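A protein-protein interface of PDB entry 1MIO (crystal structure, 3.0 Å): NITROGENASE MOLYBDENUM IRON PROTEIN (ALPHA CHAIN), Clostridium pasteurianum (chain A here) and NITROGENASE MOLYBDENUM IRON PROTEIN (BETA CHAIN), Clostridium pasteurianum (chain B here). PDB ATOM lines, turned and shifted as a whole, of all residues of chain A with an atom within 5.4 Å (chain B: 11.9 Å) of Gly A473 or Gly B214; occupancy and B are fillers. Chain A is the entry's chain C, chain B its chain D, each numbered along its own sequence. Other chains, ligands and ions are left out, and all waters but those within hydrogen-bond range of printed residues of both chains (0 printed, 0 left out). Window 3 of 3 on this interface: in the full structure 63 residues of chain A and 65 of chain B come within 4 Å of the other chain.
NZ of Lys A472 is in hydrogen-bond range of O of Pro B211 (3.2 Å). OE2 of Glu B62 is in salt-bridge range of NZ of Lys A472. The backbone carbonyl oxygen of Lys A472 is in hydrogen-bond range of the backbone NH of Gly B214 (3.4 Å). The backbone carbonyl oxygen (O) of Gly A473 sits close to the backbone carbonyl oxygen (O) of Gly B214 (3.5 Å).
OG1 of Thr B213 lies close to N of Glu B215 (3.5 Å). The side-chain sulfur (SD) of Met B65 sits close to the side-chain hydroxyl (OH) of Tyr B216, 3.7 Å away.
CG2 of Val A469 touches CE of Met B65, 3.8 Å away. Val A469 touches Tyr B216. Lys A472 touches Gly B210. NZ of Lys A472 touches OG1 of Thr B212 (3.6 Å). Ile A514 touches Thr B212 (CG2 to O, 3.5 Å). Thr B213 touches Ile A514 (O to CG2, 3.6 Å).
Lys A472 touches just these residues of chain B: Glu B62, Gly B210, Pro B211, Thr B212 and Gly B214. Gly A473 touches just one residue of chain B: Gly B214 (3.4 Å). No residue of chain B comes within 4 Å of Gly A474. No residue of chain B comes within 4 Å of Val A475. Lys B61 touches none of the printed residues of chain A. Pro B63 touches none of the printed residues of chain A. Of the printed residues of chain A, Thr B212 touches Lys A472 (3.6 Å) and Ile A514 (3.5 Å). Of the printed residues of chain A, Thr B213 touches Ile A514 (3.6 Å). Gly B214 touches just these residues of chain A: Lys A472 and Gly A473. The nearest printed residue of chain B that does not touch Gly A473 is Tyr B216 (4.6 Å). The nearest residue of chain A that does not touch Gly B214 is Ile A514 (4.1 Å).
Hydrophobic or aromatic side chains of chain B within 4 Å of the printed part of chain A: Met B65 and Tyr B216. Of the 8 printed residues of chain A, 4 touch a printed residue of chain B. Printed residues of chain A that touch a printed residue of chain B: Val A469, Lys A472, Gly A473 and Ile A514. Hydrophobic or aromatic side chains of chain A within 4 Å of the printed part of chain B: Val A469 and Ile A514. Among the printed residues, 10 pairs touch across the chains.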
ATOM      1  N   VAL A 469      15.935 -13.791 -31.696  1.00  0.00           N
ATOM      2  CA  VAL A 469      16.513 -12.503 -32.047  1.00  0.00           C
ATOM      3  C   VAL A 469      15.611 -11.495 -31.349  1.00  0.00           C
ATOM      4  O   VAL A 469      16.064 -10.667 -30.566  1.00  0.00           O
ATOM      5  CB  VAL A 469      16.474 -12.322 -33.587  1.00  0.00           C
ATOM      6  CG1 VAL A 469      16.884 -10.932 -33.956  1.00  0.00           C
ATOM      7  CG2 VAL A 469      17.453 -13.206 -34.262  1.00  0.00           C
ATOM      8  N   ILE A 470      14.299 -11.623 -31.576  1.00  0.00           N
ATOM      9  CA  ILE A 470      13.314 -10.663 -31.124  1.00  0.00           C
ATOM     10  C   ILE A 470      13.334 -10.699 -29.609  1.00  0.00           C
ATOM     11  O   ILE A 470      13.662  -9.731 -28.933  1.00  0.00           O
ATOM     12  CB  ILE A 470      11.996 -11.096 -31.818  1.00  0.00           C
ATOM     13  CG1 ILE A 470      12.193 -11.099 -33.353  1.00  0.00           C
ATOM     14  CG2 ILE A 470      10.910 -10.119 -31.539  1.00  0.00           C
ATOM     15  CD1 ILE A 470      11.146 -11.688 -34.341  1.00  0.00           C
ATOM     16  N   GLN A 471      13.171 -11.884 -29.053  1.00  0.00           N
ATOM     17  CA  GLN A 471      13.148 -12.131 -27.626  1.00  0.00           C
ATOM     18  C   GLN A 471      14.346 -11.539 -26.870  1.00  0.00           C
ATOM     19  O   GLN A 471      14.164 -10.994 -25.786  1.00  0.00           O
ATOM     20  CB  GLN A 471      13.064 -13.643 -27.484  1.00  0.00           C
ATOM     21  CG  GLN A 471      12.153 -14.214 -26.389  1.00  0.00           C
ATOM     22  CD  GLN A 471      10.688 -14.249 -26.775  1.00  0.00           C
ATOM     23  OE1 GLN A 471       9.737 -13.859 -26.082  1.00  0.00           O
ATOM     24  NE2 GLN A 471      10.485 -14.746 -27.977  1.00  0.00           N
ATOM     25  N   LYS A 472      15.560 -11.577 -27.451  1.00  0.00           N
ATOM     26  CA  LYS A 472      16.852 -11.102 -26.924  1.00  0.00           C
ATOM     27  C   LYS A 472      17.031  -9.603 -26.751  1.00  0.00           C
ATOM     28  O   LYS A 472      17.836  -9.120 -25.941  1.00  0.00           O
ATOM     29  CB  LYS A 472      17.943 -11.552 -27.823  1.00  0.00           C
ATOM     30  CG  LYS A 472      19.202 -11.955 -27.133  1.00  0.00           C
ATOM     31  CD  LYS A 472      19.430 -13.371 -27.658  1.00  0.00           C
ATOM     32  CE  LYS A 472      20.586 -14.105 -27.043  1.00  0.00           C
ATOM     33  NZ  LYS A 472      20.391 -14.189 -25.617  1.00  0.00           N
ATOM     34  N   GLY A 473      16.309  -8.896 -27.609  1.00  0.00           N
ATOM     35  CA  GLY A 473      16.249  -7.470 -27.561  1.00  0.00           C
ATOM     36  C   GLY A 473      15.103  -7.017 -26.666  1.00  0.00           C
ATOM     37  O   GLY A 473      14.786  -5.826 -26.625  1.00  0.00           O
ATOM     38  N   GLY A 474      14.399  -7.896 -25.970  1.00  0.00           N
ATOM     39  CA  GLY A 474      13.374  -7.466 -25.034  1.00  0.00           C
ATOM     40  C   GLY A 474      11.951  -7.377 -25.584  1.00  0.00           C
ATOM     41  O   GLY A 474      11.092  -6.763 -24.942  1.00  0.00           O
ATOM     42  N   VAL A 475      11.657  -7.992 -26.736  1.00  0.00           N
ATOM     43  CA  VAL A 475      10.322  -8.004 -27.289  1.00  0.00           C
ATOM     44  C   VAL A 475       9.992  -9.467 -27.593  1.00  0.00           C
ATOM     45  O   VAL A 475      10.809 -10.333 -27.895  1.00  0.00           O
ATOM     46  CB  VAL A 475      10.224  -6.993 -28.573  1.00  0.00           C
ATOM     47  CG1 VAL A 475      11.292  -7.215 -29.649  1.00  0.00           C
ATOM     48  CG2 VAL A 475       8.853  -7.182 -29.255  1.00  0.00           C
ATOM     49  N   ILE A 514      15.643  -7.228 -16.808  1.00  0.00           N
ATOM     50  CA  ILE A 514      16.783  -7.531 -17.652  1.00  0.00           C
ATOM     51  C   ILE A 514      17.974  -6.642 -17.309  1.00  0.00           C
ATOM     52  O   ILE A 514      19.130  -7.054 -17.431  1.00  0.00           O
ATOM     53  CB  ILE A 514      16.411  -7.374 -19.161  1.00  0.00           C
ATOM     54  CG1 ILE A 514      15.229  -8.215 -19.626  1.00  0.00           C
ATOM     55  CG2 ILE A 514      17.557  -7.924 -19.944  1.00  0.00           C
ATOM     56  CD1 ILE A 514      14.895  -8.200 -21.134  1.00  0.00           C
ATOM     57  N   LYS B  61      18.433 -22.916 -27.717  1.00  0.00           N
ATOM     58  CA  LYS B  61      17.405 -21.914 -27.458  1.00  0.00           C
ATOM     59  C   LYS B  61      18.102 -20.534 -27.594  1.00  0.00           C
ATOM     60  O   LYS B  61      18.189 -19.637 -26.698  1.00  0.00           O
ATOM     61  CB  LYS B  61      16.775 -22.217 -26.049  1.00  0.00           C
ATOM     62  CG  LYS B  61      15.982 -23.537 -25.858  1.00  0.00           C
ATOM     63  CD  LYS B  61      14.604 -23.769 -26.598  1.00  0.00           C
ATOM     64  CE  LYS B  61      14.488 -24.297 -28.108  1.00  0.00           C
ATOM     65  NZ  LYS B  61      13.186 -24.234 -28.805  1.00  0.00           N
ATOM     66  N   GLU B  62      18.703 -20.417 -28.784  1.00  0.00           N
ATOM     67  CA  GLU B  62      19.667 -19.375 -29.145  1.00  0.00           C
ATOM     68  C   GLU B  62      19.570 -19.029 -30.642  1.00  0.00           C
ATOM     69  O   GLU B  62      18.801 -19.712 -31.331  1.00  0.00           O
ATOM     70  CB  GLU B  62      21.061 -19.912 -28.782  1.00  0.00           C
ATOM     71  CG  GLU B  62      22.085 -18.995 -28.154  1.00  0.00           C
ATOM     72  CD  GLU B  62      21.648 -18.252 -26.906  1.00  0.00           C
ATOM     73  OE1 GLU B  62      21.174 -18.887 -25.961  1.00  0.00           O
ATOM     74  OE2 GLU B  62      21.830 -17.039 -26.862  1.00  0.00           O
ATOM     75  N   PRO B  63      20.205 -17.956 -31.181  1.00  0.00           N
ATOM     76  CA  PRO B  63      20.244 -17.682 -32.604  1.00  0.00           C
ATOM     77  C   PRO B  63      21.462 -18.197 -33.347  1.00  0.00           C
ATOM     78  O   PRO B  63      22.602 -17.980 -32.923  1.00  0.00           O
ATOM     79  CB  PRO B  63      20.113 -16.166 -32.710  1.00  0.00           C
ATOM     80  CG  PRO B  63      19.910 -15.622 -31.314  1.00  0.00           C
ATOM     81  CD  PRO B  63      20.534 -16.702 -30.490  1.00  0.00           C
ATOM     82  N   MET B  65      22.864 -17.695 -37.084  1.00  0.00           N
ATOM     83  CA  MET B  65      22.766 -16.650 -38.077  1.00  0.00           C
ATOM     84  C   MET B  65      23.617 -17.161 -39.218  1.00  0.00           C
ATOM     85  O   MET B  65      24.766 -17.508 -38.939  1.00  0.00           O
ATOM     86  CB  MET B  65      23.329 -15.383 -37.431  1.00  0.00           C
ATOM     87  CG  MET B  65      22.736 -14.060 -37.879  1.00  0.00           C
ATOM     88  SD  MET B  65      20.940 -13.771 -37.798  1.00  0.00           S
ATOM     89  CE  MET B  65      20.457 -14.415 -36.223  1.00  0.00           C
ATOM     90  N   GLY B 210      24.420 -17.648 -23.321  1.00  0.00           N
ATOM     91  CA  GLY B 210      24.657 -16.246 -23.090  1.00  0.00           C
ATOM     92  C   GLY B 210      23.424 -15.439 -22.767  1.00  0.00           C
ATOM     93  O   GLY B 210      22.309 -15.984 -22.689  1.00  0.00           O
ATOM     94  N   PRO B 211      23.728 -14.152 -22.494  1.00  0.00           N
ATOM     95  CA  PRO B 211      22.917 -13.229 -21.736  1.00  0.00           C
ATOM     96  C   PRO B 211      21.754 -12.623 -22.446  1.00  0.00           C
ATOM     97  O   PRO B 211      21.962 -12.268 -23.585  1.00  0.00           O
ATOM     98  CB  PRO B 211      23.867 -12.150 -21.275  1.00  0.00           C
ATOM     99  CG  PRO B 211      25.242 -12.711 -21.486  1.00  0.00           C
ATOM    100  CD  PRO B 211      25.028 -13.518 -22.745  1.00  0.00           C
ATOM    101  N   THR B 212      20.550 -12.491 -21.924  1.00  0.00           N
ATOM    102  CA  THR B 212      19.610 -11.601 -22.551  1.00  0.00           C
ATOM    103  C   THR B 212      20.012 -10.309 -21.822  1.00  0.00           C
ATOM    104  O   THR B 212      20.004 -10.305 -20.582  1.00  0.00           O
ATOM    105  CB  THR B 212      18.176 -12.083 -22.264  1.00  0.00           C
ATOM    106  OG1 THR B 212      17.897 -13.060 -23.261  1.00  0.00           O
ATOM    107  CG2 THR B 212      17.134 -11.018 -22.362  1.00  0.00           C
ATOM    108  N   THR B 213      20.531  -9.287 -22.562  1.00  0.00           N
ATOM    109  CA  THR B 213      20.886  -7.980 -21.980  1.00  0.00           C
ATOM    110  C   THR B 213      19.942  -6.883 -22.407  1.00  0.00           C
ATOM    111  O   THR B 213      19.832  -5.859 -21.725  1.00  0.00           O
ATOM    112  CB  THR B 213      22.352  -7.424 -22.332  1.00  0.00           C
ATOM    113  OG1 THR B 213      22.563  -7.195 -23.758  1.00  0.00           O
ATOM    114  CG2 THR B 213      23.351  -8.398 -21.684  1.00  0.00           C
ATOM    115  N   GLY B 214      19.265  -7.098 -23.543  1.00  0.00           N
ATOM    116  CA  GLY B 214      18.351  -6.121 -24.102  1.00  0.00           C
ATOM    117  C   GLY B 214      18.874  -5.611 -25.438  1.00  0.00           C
ATOM    118  O   GLY B 214      18.127  -4.999 -26.186  1.00  0.00           O
ATOM    119  N   GLU B 215      20.134  -5.758 -25.823  1.00  0.00           N
ATOM    120  CA  GLU B 215      20.531  -5.334 -27.154  1.00  0.00           C
ATOM    121  C   GLU B 215      20.856  -6.634 -27.897  1.00  0.00           C
ATOM    122  O   GLU B 215      21.390  -7.557 -27.282  1.00  0.00           O
ATOM    123  CB  GLU B 215      21.739  -4.374 -27.025  1.00  0.00           C
ATOM    124  CG  GLU B 215      22.872  -4.880 -26.127  1.00  0.00           C
ATOM    125  CD  GLU B 215      23.825  -3.820 -25.566  1.00  0.00           C
ATOM    126  OE1 GLU B 215      23.434  -3.122 -24.618  1.00  0.00           O
ATOM    127  OE2 GLU B 215      24.958  -3.715 -26.057  1.00  0.00           O
ATOM    128  N   TYR B 216      20.502  -6.858 -29.154  1.00  0.00           N
ATOM    129  CA  TYR B 216      20.915  -8.063 -29.849  1.00  0.00           C
ATOM    130  C   TYR B 216      22.168  -7.739 -30.704  1.00  0.00           C
ATOM    131  O   TYR B 216      22.209  -6.696 -31.377  1.00  0.00           O
ATOM    132  CB  TYR B 216      19.695  -8.610 -30.730  1.00  0.00           C
ATOM    133  CG  TYR B 216      20.089  -9.631 -31.807  1.00  0.00           C
ATOM    134  CD1 TYR B 216      20.595 -10.865 -31.447  1.00  0.00           C
ATOM    135  CD2 TYR B 216      20.102  -9.272 -33.133  1.00  0.00           C
ATOM    136  CE1 TYR B 216      21.150 -11.724 -32.373  1.00  0.00           C
ATOM    137  CE2 TYR B 216      20.645 -10.133 -34.061  1.00  0.00           C
ATOM    138  CZ  TYR B 216      21.172 -11.343 -33.677  1.00  0.00           C
ATOM    139  OH  TYR B 216      21.788 -12.146 -34.602  1.00  0.00           O
ATOM    140  N   LYS B 217      23.203  -8.607 -30.709  1.00  0.00           N
ATOM    141  CA  LYS B 217      24.321  -8.467 -31.635  1.00  0.00           C
ATOM    142  C   LYS B 217      24.452  -9.671 -32.584  1.00  0.00           C
ATOM    143  O   LYS B 217      24.669 -10.804 -32.160  1.00  0.00           O
ATOM    144  CB  LYS B 217      25.680  -8.306 -30.910  1.00  0.00           C
ATOM    145  CG  LYS B 217      25.971  -7.140 -29.945  1.00  0.00           C
ATOM    146  CD  LYS B 217      25.679  -7.528 -28.483  1.00  0.00           C
ATOM    147  CE  LYS B 217      26.288  -6.564 -27.453  1.00  0.00           C
ATOM    148  NZ  LYS B 217      27.705  -6.335 -27.678  1.00  0.00           N
ATOM    149  N   MET B 218      24.366  -9.425 -33.907  1.00  0.00           N
ATOM    150  CA  MET B 218      24.515 -10.424 -34.976  1.00  0.00           C
ATOM    151  C   MET B 218      25.793 -11.248 -34.732  1.00  0.00           C
ATOM    152  O   MET B 218      25.895 -12.457 -34.994  1.00  0.00           O
ATOM    153  CB  MET B 218      24.609  -9.733 -36.343  1.00  0.00           C
ATOM    154  CG  MET B 218      24.759 -10.718 -37.506  1.00  0.00           C
ATOM    155  SD  MET B 218      24.037 -10.125 -39.022  1.00  0.00           S
ATOM    156  CE  MET B 218      24.249 -11.333 -40.312  1.00  0.00           C
ATOM    157  N   PRO B 220      27.713 -11.996 -31.519  1.00  0.00           N
ATOM    158  CA  PRO B 220      28.015 -12.067 -30.098  1.00  0.00           C
ATOM    159  C   PRO B 220      29.524 -11.982 -29.896  1.00  0.00           C
ATOM    160  O   PRO B 220      30.329 -12.172 -30.820  1.00  0.00           O
ATOM    161  CB  PRO B 220      27.413 -13.381 -29.677  1.00  0.00           C
ATOM    162  CG  PRO B 220      26.362 -13.690 -30.715  1.00  0.00           C
ATOM    163  CD  PRO B 220      27.040 -13.217 -31.972  1.00  0.00           C
ATOM    164  N   GLU B 221      29.935 -11.702 -28.664  1.00  0.00           N
ATOM    165  CA  GLU B 221      31.356 -11.600 -28.333  1.00  0.00           C
ATOM    166  C   GLU B 221      32.258 -12.777 -27.947  1.00  0.00           C
ATOM    167  O   GLU B 221      33.420 -12.535 -27.628  1.00  0.00           O
ATOM    168  CB  GLU B 221      31.510 -10.567 -27.267  1.00  0.00           C
ATOM    169  CG  GLU B 221      30.771 -10.835 -26.016  1.00  0.00           C
ATOM    170  CD  GLU B 221      30.448  -9.520 -25.338  1.00  0.00           C
ATOM    171  OE1 GLU B 221      31.331  -8.938 -24.680  1.00  0.00           O
ATOM    172  OE2 GLU B 221      29.295  -9.096 -25.490  1.00  0.00           O
